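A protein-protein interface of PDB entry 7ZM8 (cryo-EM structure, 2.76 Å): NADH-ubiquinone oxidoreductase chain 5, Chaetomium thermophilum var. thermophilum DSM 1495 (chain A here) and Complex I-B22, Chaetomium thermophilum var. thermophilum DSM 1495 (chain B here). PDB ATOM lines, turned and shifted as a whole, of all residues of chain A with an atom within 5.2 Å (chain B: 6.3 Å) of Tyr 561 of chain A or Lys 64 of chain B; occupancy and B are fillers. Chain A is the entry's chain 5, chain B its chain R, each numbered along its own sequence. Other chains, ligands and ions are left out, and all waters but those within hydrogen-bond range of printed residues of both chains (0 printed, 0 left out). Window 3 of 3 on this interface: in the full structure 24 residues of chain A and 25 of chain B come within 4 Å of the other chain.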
ATOM      1  N   PHE A 554      26.629  -4.757   6.886  1.00  0.00           N
ATOM      2  CA  PHE A 554      25.832  -5.481   5.871  1.00  0.00           C
ATOM      3  C   PHE A 554      24.395  -5.662   6.343  1.00  0.00           C
ATOM      4  O   PHE A 554      23.479  -5.390   5.566  1.00  0.00           O
ATOM      5  CB  PHE A 554      26.454  -6.839   5.544  1.00  0.00           C
ATOM      6  CG  PHE A 554      25.749  -7.610   4.460  1.00  0.00           C
ATOM      7  CD1 PHE A 554      25.838  -7.216   3.136  1.00  0.00           C
ATOM      8  CD2 PHE A 554      24.990  -8.726   4.764  1.00  0.00           C
ATOM      9  CE1 PHE A 554      25.185  -7.925   2.139  1.00  0.00           C
ATOM     10  CE2 PHE A 554      24.337  -9.434   3.769  1.00  0.00           C
ATOM     11  CZ  PHE A 554      24.437  -9.033   2.458  1.00  0.00           C
ATOM     12  N   LYS A 555      24.199  -6.104   7.575  1.00  0.00           N
ATOM     13  CA  LYS A 555      22.825  -6.430   8.017  1.00  0.00           C
ATOM     14  C   LYS A 555      22.034  -5.154   8.308  1.00  0.00           C
ATOM     15  O   LYS A 555      20.794  -5.222   8.302  1.00  0.00           O
ATOM     16  CB  LYS A 555      22.903  -7.357   9.231  1.00  0.00           C
ATOM     17  CG  LYS A 555      23.613  -8.679   8.984  1.00  0.00           C
ATOM     18  CD  LYS A 555      23.726  -9.545  10.214  1.00  0.00           C
ATOM     19  CE  LYS A 555      24.636  -8.965  11.269  1.00  0.00           C
ATOM     20  NZ  LYS A 555      24.717  -9.856  12.445  1.00  0.00           N
ATOM     21  N   SER A 557      22.239  -2.519   6.360  1.00  0.00           N
ATOM     22  CA  SER A 557      21.865  -1.968   5.071  1.00  0.00           C
ATOM     23  C   SER A 557      20.571  -2.627   4.626  1.00  0.00           C
ATOM     24  O   SER A 557      20.317  -3.788   4.951  1.00  0.00           O
ATOM     25  CB  SER A 557      22.969  -2.201   4.041  1.00  0.00           C
ATOM     26  OG  SER A 557      23.003  -3.551   3.622  1.00  0.00           O
ATOM     27  N   ARG A 558      19.735  -1.879   3.905  1.00  0.00           N
ATOM     28  CA  ARG A 558      18.451  -2.443   3.507  1.00  0.00           C
ATOM     29  C   ARG A 558      18.631  -3.595   2.537  1.00  0.00           C
ATOM     30  O   ARG A 558      17.790  -4.499   2.489  1.00  0.00           O
ATOM     31  CB  ARG A 558      17.548  -1.374   2.896  1.00  0.00           C
ATOM     32  CG  ARG A 558      17.185  -0.267   3.849  1.00  0.00           C
ATOM     33  CD  ARG A 558      16.309  -0.763   4.978  1.00  0.00           C
ATOM     34  NE  ARG A 558      15.325  -1.743   4.541  1.00  0.00           N
ATOM     35  CZ  ARG A 558      14.557  -2.442   5.367  1.00  0.00           C
ATOM     36  NH1 ARG A 558      14.657  -2.271   6.676  1.00  0.00           N
ATOM     37  NH2 ARG A 558      13.685  -3.309   4.882  1.00  0.00           N
ATOM     38  N   PHE A 559      19.712  -3.580   1.756  1.00  0.00           N
ATOM     39  CA  PHE A 559      20.002  -4.704   0.874  1.00  0.00           C
ATOM     40  C   PHE A 559      20.324  -5.953   1.677  1.00  0.00           C
ATOM     41  O   PHE A 559      19.741  -7.018   1.451  1.00  0.00           O
ATOM     42  CB  PHE A 559      21.156  -4.345  -0.066  1.00  0.00           C
ATOM     43  CG  PHE A 559      21.539  -5.450  -1.011  1.00  0.00           C
ATOM     44  CD1 PHE A 559      22.436  -6.432  -0.629  1.00  0.00           C
ATOM     45  CD2 PHE A 559      20.980  -5.521  -2.274  1.00  0.00           C
ATOM     46  CE1 PHE A 559      22.779  -7.449  -1.491  1.00  0.00           C
ATOM     47  CE2 PHE A 559      21.320  -6.538  -3.140  1.00  0.00           C
ATOM     48  CZ  PHE A 559      22.222  -7.502  -2.747  1.00  0.00           C
ATOM     49  N   GLY A 560      21.245  -5.836   2.634  1.00  0.00           N
ATOM     50  CA  GLY A 560      21.615  -6.967   3.461  1.00  0.00           C
ATOM     51  C   GLY A 560      20.571  -7.351   4.481  1.00  0.00           C
ATOM     52  O   GLY A 560      20.560  -8.496   4.935  1.00  0.00           O
ATOM     53  N   TYR A 561      19.699  -6.418   4.860  1.00  0.00           N
ATOM     54  CA  TYR A 561      18.591  -6.761   5.742  1.00  0.00           C
ATOM     55  C   TYR A 561      17.670  -7.768   5.074  1.00  0.00           C
ATOM     56  O   TYR A 561      17.190  -8.708   5.716  1.00  0.00           O
ATOM     57  CB  TYR A 561      17.825  -5.497   6.134  1.00  0.00           C
ATOM     58  CG  TYR A 561      16.567  -5.738   6.934  1.00  0.00           C
ATOM     59  CD1 TYR A 561      15.356  -5.972   6.302  1.00  0.00           C
ATOM     60  CD2 TYR A 561      16.588  -5.723   8.322  1.00  0.00           C
ATOM     61  CE1 TYR A 561      14.214  -6.191   7.021  1.00  0.00           C
ATOM     62  CE2 TYR A 561      15.448  -5.940   9.046  1.00  0.00           C
ATOM     63  CZ  TYR A 561      14.263  -6.169   8.392  1.00  0.00           C
ATOM     64  OH  TYR A 561      13.111  -6.388   9.101  1.00  0.00           O
ATOM     65  N   ASN A 562      17.411  -7.581   3.781  1.00  0.00           N
ATOM     66  CA  ASN A 562      16.536  -8.492   3.058  1.00  0.00           C
ATOM     67  C   ASN A 562      17.234  -9.808   2.753  1.00  0.00           C
ATOM     68  O   ASN A 562      16.600 -10.868   2.766  1.00  0.00           O
ATOM     69  CB  ASN A 562      16.054  -7.828   1.772  1.00  0.00           C
ATOM     70  CG  ASN A 562      15.103  -6.689   2.035  1.00  0.00           C
ATOM     71  OD1 ASN A 562      13.903  -6.894   2.179  1.00  0.00           O
ATOM     72  ND2 ASN A 562      15.636  -5.480   2.120  1.00  0.00           N
ATOM     73  N   ILE A 563      18.542  -9.760   2.545  1.00  0.00           N
ATOM     74  CA  ILE A 563      19.310 -10.977   2.165  1.00  0.00           C
ATOM     75  C   ILE A 563      19.493 -11.828   3.421  1.00  0.00           C
ATOM     76  O   ILE A 563      19.444 -13.055   3.309  1.00  0.00           O
ATOM     77  CB  ILE A 563      20.623 -10.604   1.452  1.00  0.00           C
ATOM     78  CG1 ILE A 563      20.354  -9.971   0.086  1.00  0.00           C
ATOM     79  CG2 ILE A 563      21.550 -11.801   1.330  1.00  0.00           C
ATOM     80  CD1 ILE A 563      19.502 -10.821  -0.824  1.00  0.00           C
ATOM     81  N   PHE A 564      19.571 -11.187   4.587  1.00  0.00           N
ATOM     82  CA  PHE A 564      19.819 -11.943   5.836  1.00  0.00           C
ATOM     83  C   PHE A 564      18.499 -12.589   6.221  1.00  0.00           C
ATOM     84  O   PHE A 564      18.522 -13.759   6.611  1.00  0.00           O
ATOM     85  CB  PHE A 564      20.302 -11.057   6.988  1.00  0.00           C
ATOM     86  CG  PHE A 564      20.539 -11.772   8.295  1.00  0.00           C
ATOM     87  CD1 PHE A 564      19.489 -12.073   9.149  1.00  0.00           C
ATOM     88  CD2 PHE A 564      21.816 -12.140   8.680  1.00  0.00           C
ATOM     89  CE1 PHE A 564      19.705 -12.740  10.342  1.00  0.00           C
ATOM     90  CE2 PHE A 564      22.033 -12.795   9.881  1.00  0.00           C
ATOM     91  CZ  PHE A 564      20.979 -13.092  10.710  1.00  0.00           C
ATOM     92  N   GLY A 565      17.394 -11.864   6.068  1.00  0.00           N
ATOM     93  CA  GLY A 565      16.111 -12.430   6.424  1.00  0.00           C
ATOM     94  C   GLY A 565      15.599 -13.436   5.419  1.00  0.00           C
ATOM     95  O   GLY A 565      14.803 -14.310   5.765  1.00  0.00           O
ATOM     96  N   PHE A 566      16.042 -13.332   4.167  1.00  0.00           N
ATOM     97  CA  PHE A 566      15.624 -14.292   3.155  1.00  0.00           C
ATOM     98  C   PHE A 566      16.176 -15.675   3.459  1.00  0.00           C
ATOM     99  O   PHE A 566      15.455 -16.676   3.383  1.00  0.00           O
ATOM    100  CB  PHE A 566      16.080 -13.827   1.774  1.00  0.00           C
ATOM    101  CG  PHE A 566      15.678 -14.744   0.656  1.00  0.00           C
ATOM    102  CD1 PHE A 566      14.454 -14.595   0.031  1.00  0.00           C
ATOM    103  CD2 PHE A 566      16.531 -15.746   0.218  1.00  0.00           C
ATOM    104  CE1 PHE A 566      14.088 -15.426  -0.997  1.00  0.00           C
ATOM    105  CE2 PHE A 566      16.165 -16.578  -0.811  1.00  0.00           C
ATOM    106  CZ  PHE A 566      14.943 -16.416  -1.419  1.00  0.00           C
ATOM    107  N   TRP B  21      20.596  -8.093  16.359  1.00  0.00           N
ATOM    108  CA  TRP B  21      21.334  -7.926  15.115  1.00  0.00           C
ATOM    109  C   TRP B  21      22.832  -7.866  15.359  1.00  0.00           C
ATOM    110  O   TRP B  21      23.612  -8.478  14.625  1.00  0.00           O
ATOM    111  CB  TRP B  21      20.859  -6.666  14.405  1.00  0.00           C
ATOM    112  CG  TRP B  21      19.563  -6.837  13.736  1.00  0.00           C
ATOM    113  CD1 TRP B  21      18.374  -6.287  14.096  1.00  0.00           C
ATOM    114  CD2 TRP B  21      19.312  -7.615  12.573  1.00  0.00           C
ATOM    115  NE1 TRP B  21      17.392  -6.678  13.228  1.00  0.00           N
ATOM    116  CE2 TRP B  21      17.944  -7.499  12.283  1.00  0.00           C
ATOM    117  CE3 TRP B  21      20.113  -8.406  11.749  1.00  0.00           C
ATOM    118  CZ2 TRP B  21      17.362  -8.141  11.203  1.00  0.00           C
ATOM    119  CZ3 TRP B  21      19.537  -9.038  10.688  1.00  0.00           C
ATOM    120  CH2 TRP B  21      18.175  -8.903  10.417  1.00  0.00           C
ATOM    121  N   GLU B  59       7.392   2.760  16.832  1.00  0.00           N
ATOM    122  CA  GLU B  59       6.845   1.449  16.525  1.00  0.00           C
ATOM    123  C   GLU B  59       7.065   1.070  15.070  1.00  0.00           C
ATOM    124  O   GLU B  59       7.144  -0.122  14.756  1.00  0.00           O
ATOM    125  CB  GLU B  59       5.353   1.425  16.860  1.00  0.00           C
ATOM    126  CG  GLU B  59       4.727   0.038  16.868  1.00  0.00           C
ATOM    127  CD  GLU B  59       5.097  -0.757  18.103  1.00  0.00           C
ATOM    128  OE1 GLU B  59       5.382  -0.134  19.148  1.00  0.00           O
ATOM    129  OE2 GLU B  59       5.101  -2.004  18.032  1.00  0.00           O
ATOM    130  N   LYS B  60       7.164   2.055  14.177  1.00  0.00           N
ATOM    131  CA  LYS B  60       7.478   1.775  12.782  1.00  0.00           C
ATOM    132  C   LYS B  60       8.919   1.337  12.602  1.00  0.00           C
ATOM    133  O   LYS B  60       9.206   0.509  11.734  1.00  0.00           O
ATOM    134  CB  LYS B  60       7.204   3.002  11.915  1.00  0.00           C
ATOM    135  CG  LYS B  60       5.908   3.710  12.222  1.00  0.00           C
ATOM    136  CD  LYS B  60       5.487   4.610  11.072  1.00  0.00           C
ATOM    137  CE  LYS B  60       4.978   3.797   9.893  1.00  0.00           C
ATOM    138  NZ  LYS B  60       3.911   2.843  10.300  1.00  0.00           N
ATOM    139  N   LEU B  61       9.831   1.865  13.428  1.00  0.00           N
ATOM    140  CA  LEU B  61      11.283   1.596  13.225  1.00  0.00           C
ATOM    141  C   LEU B  61      11.630   0.272  13.897  1.00  0.00           C
ATOM    142  O   LEU B  61      12.691  -0.294  13.601  1.00  0.00           O
ATOM    143  CB  LEU B  61      12.095   2.746  13.818  1.00  0.00           C
ATOM    144  CG  LEU B  61      12.176   4.014  12.978  1.00  0.00           C
ATOM    145  CD1 LEU B  61      12.841   5.127  13.771  1.00  0.00           C
ATOM    146  CD2 LEU B  61      12.934   3.753  11.687  1.00  0.00           C
ATOM    147  N   LEU B  62      10.721  -0.215  14.728  1.00  0.00           N
ATOM    148  CA  LEU B  62      10.949  -1.485  15.447  1.00  0.00           C
ATOM    149  C   LEU B  62      10.468  -2.577  14.506  1.00  0.00           C
ATOM    150  O   LEU B  62      11.042  -3.673  14.556  1.00  0.00           O
ATOM    151  CB  LEU B  62      10.173  -1.448  16.765  1.00  0.00           C
ATOM    152  CG  LEU B  62      10.975  -1.075  18.012  1.00  0.00           C
ATOM    153  CD1 LEU B  62      11.885  -2.213  18.438  1.00  0.00           C
ATOM    154  CD2 LEU B  62      11.778   0.195  17.791  1.00  0.00           C
ATOM    155  N   GLU B  63       9.447  -2.296  13.702  1.00  0.00           N
ATOM    156  CA  GLU B  63       9.033  -3.225  12.660  1.00  0.00           C
ATOM    157  C   GLU B  63       9.941  -3.167  11.447  1.00  0.00           C
ATOM    158  O   GLU B  63      10.214  -4.201  10.834  1.00  0.00           O
ATOM    159  CB  GLU B  63       7.601  -2.928  12.220  1.00  0.00           C
ATOM    160  CG  GLU B  63       6.556  -3.151  13.289  1.00  0.00           C
ATOM    161  CD  GLU B  63       6.417  -4.607  13.681  1.00  0.00           C
ATOM    162  OE1 GLU B  63       6.686  -5.483  12.833  1.00  0.00           O
ATOM    163  OE2 GLU B  63       6.036  -4.874  14.840  1.00  0.00           O
ATOM    164  N   LYS B  64      10.409  -1.968  11.091  1.00  0.00           N
ATOM    165  CA  LYS B  64      11.248  -1.794   9.914  1.00  0.00           C
ATOM    166  C   LYS B  64      12.551  -2.562  10.032  1.00  0.00           C
ATOM    167  O   LYS B  64      13.103  -3.003   9.018  1.00  0.00           O
ATOM    168  CB  LYS B  64      11.535  -0.312   9.702  1.00  0.00           C
ATOM    169  CG  LYS B  64      12.332  -0.005   8.454  1.00  0.00           C
ATOM    170  CD  LYS B  64      12.532   1.479   8.283  1.00  0.00           C
ATOM    171  CE  LYS B  64      13.251   1.779   6.985  1.00  0.00           C
ATOM    172  NZ  LYS B  64      14.650   1.283   7.019  1.00  0.00           N
ATOM    173  N   TRP B  65      13.015  -2.738  11.269  1.00  0.00           N
ATOM    174  CA  TRP B  65      14.337  -3.366  11.504  1.00  0.00           C
ATOM    175  C   TRP B  65      14.177  -4.619  12.351  1.00  0.00           C
ATOM    176  O   TRP B  65      15.153  -5.013  12.980  1.00  0.00           O
ATOM    177  CB  TRP B  65      15.316  -2.358  12.097  1.00  0.00           C
ATOM    178  CG  TRP B  65      15.676  -1.281  11.125  1.00  0.00           C
ATOM    179  CD1 TRP B  65      15.160  -0.021  11.056  1.00  0.00           C
ATOM    180  CD2 TRP B  65      16.619  -1.391  10.048  1.00  0.00           C
ATOM    181  NE1 TRP B  65      15.726   0.664  10.017  1.00  0.00           N
ATOM    182  CE2 TRP B  65      16.622  -0.151   9.378  1.00  0.00           C
ATOM    183  CE3 TRP B  65      17.463  -2.408   9.593  1.00  0.00           C
ATOM    184  CZ2 TRP B  65      17.446   0.096   8.283  1.00  0.00           C
ATOM    185  CZ3 TRP B  65      18.270  -2.166   8.506  1.00  0.00           C
ATOM    186  CH2 TRP B  65      18.258  -0.930   7.863  1.00  0.00           C
ATOM    187  N   LYS B  66      12.992  -5.220  12.356  1.00  0.00           N
ATOM    188  CA  LYS B  66      12.744  -6.371  13.205  1.00  0.00           C
ATOM    189  C   LYS B  66      13.636  -7.535  12.796  1.00  0.00           C
ATOM    190  O   LYS B  66      13.984  -7.694  11.625  1.00  0.00           O
ATOM    191  CB  LYS B  66      11.269  -6.772  13.140  1.00  0.00           C
ATOM    192  CG  LYS B  66      10.833  -7.396  11.838  1.00  0.00           C
ATOM    193  CD  LYS B  66       9.335  -7.295  11.672  1.00  0.00           C
ATOM    194  CE  LYS B  66       8.877  -7.836  10.326  1.00  0.00           C
ATOM    195  NZ  LYS B  66       8.768  -9.317  10.305  1.00  0.00           N
ATOM    196  N   HIS B  67      14.026  -8.329  13.767  1.00  0.00           N
ATOM    197  CA  HIS B  67      14.869  -9.477  13.488  1.00  0.00           C
ATOM    198  C   HIS B  67      14.015 -10.659  13.035  1.00  0.00           C
ATOM    199  O   HIS B  67      12.933 -10.882  13.580  1.00  0.00           O
ATOM    200  CB  HIS B  67      15.677  -9.861  14.721  1.00  0.00           C
ATOM    201  CG  HIS B  67      16.956 -10.568  14.405  1.00  0.00           C
ATOM    202  ND1 HIS B  67      17.002 -11.890  14.033  1.00  0.00           N
ATOM    203  CD2 HIS B  67      18.234 -10.129  14.389  1.00  0.00           C
ATOM    204  CE1 HIS B  67      18.253 -12.239  13.806  1.00  0.00           C
ATOM    205  NE2 HIS B  67      19.021 -11.188  14.017  1.00  0.00           N
ATOM    206  N   PRO B  68      14.469 -11.417  12.033  1.00  0.00           N
ATOM    207  CA  PRO B  68      13.721 -12.615  11.626  1.00  0.00           C
ATOM    208  C   PRO B  68      13.604 -13.651  12.725  1.00  0.00           C
ATOM    209  O   PRO B  68      12.622 -14.400  12.758  1.00  0.00           O
ATOM    210  CB  PRO B  68      14.532 -13.148  10.437  1.00  0.00           C
ATOM    211  CG  PRO B  68      15.465 -12.073  10.067  1.00  0.00           C
ATOM    212  CD  PRO B  68      15.708 -11.254  11.261  1.00  0.00           C
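The backbone carbonyl oxygen (O) of Trp 21 of chain B is in hydrogen-bond range of the side-chain amino group (NZ) of Lys 555 of chain A. O of Lys 64 of chain B lies within hydrogen-bond range of NH1 of Arg 558 of chain A (2.9 Å). The backbone carbonyl oxygen of Lys 64 of chain B lies within hydrogen-bond range of the side-chain hydroxyl of Tyr 561 of chain A, at 3.4 Å. The backbone carbonyl oxygen (O) of Lys 66 of chain B sits at hydrogen-bond distance from the side-chain hydroxyl (OH) of Tyr 561 of chain A (3.0 Å).
The indole nitrogen (NE1) of Trp 21 of chain B lies within hydrogen-bond range of the backbone carbonyl oxygen (O) of Trp 65 of chain B (2.8 Å).
Lys 555 of chain A touches Trp 65 of chain B. Arg 558 of chain A touches Trp 65 of chain B (CD to CH2, 3.5 Å). CE2 of Tyr 561 of chain A touches CZ2 of Trp 21 of chain B, at 3.6 Å. CE3 of Trp 65 of chain B touches CD2 of Tyr 561 of chain A (3.7 Å). CZ3 of Trp 21 of chain B touches CD1 of Phe 564 of chain A, at 3.4 Å. Phe 564 of chain A touches His 67 of chain B. Gly 565 of chain A touches Pro 68 of chain B.
Tyr 561 of chain A touches just these residues of chain B: Trp 21 (3.6 Å), Lys 64 (3.4 Å), Trp 65 (3.7 Å) and Lys 66 (3.0 Å). Lys 64 of chain B touches two residues of chain A. Of the printed residues of chain A, Lys 66 of chain B touches Tyr 561 (3.0 Å). Of the printed residues of chain A, His 67 of chain B touches Phe 564 (3.8 Å).
Hydrophobic or aromatic side chains of chain B within 4 Å of the printed part of chain A: Trp 21, Trp 65, His 67 and Pro 68. Printed residues of chain A that touch a printed residue of chain B: Lys 555, Arg 558, Tyr 561, Phe 564 and Gly 565. Among the printed residues, 11 pairs touch across the chains. Among the printed residues, no Asp or Glu carboxylate lies within 4 Å of a Lys or Arg side-chain nitrogen of the other chain.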
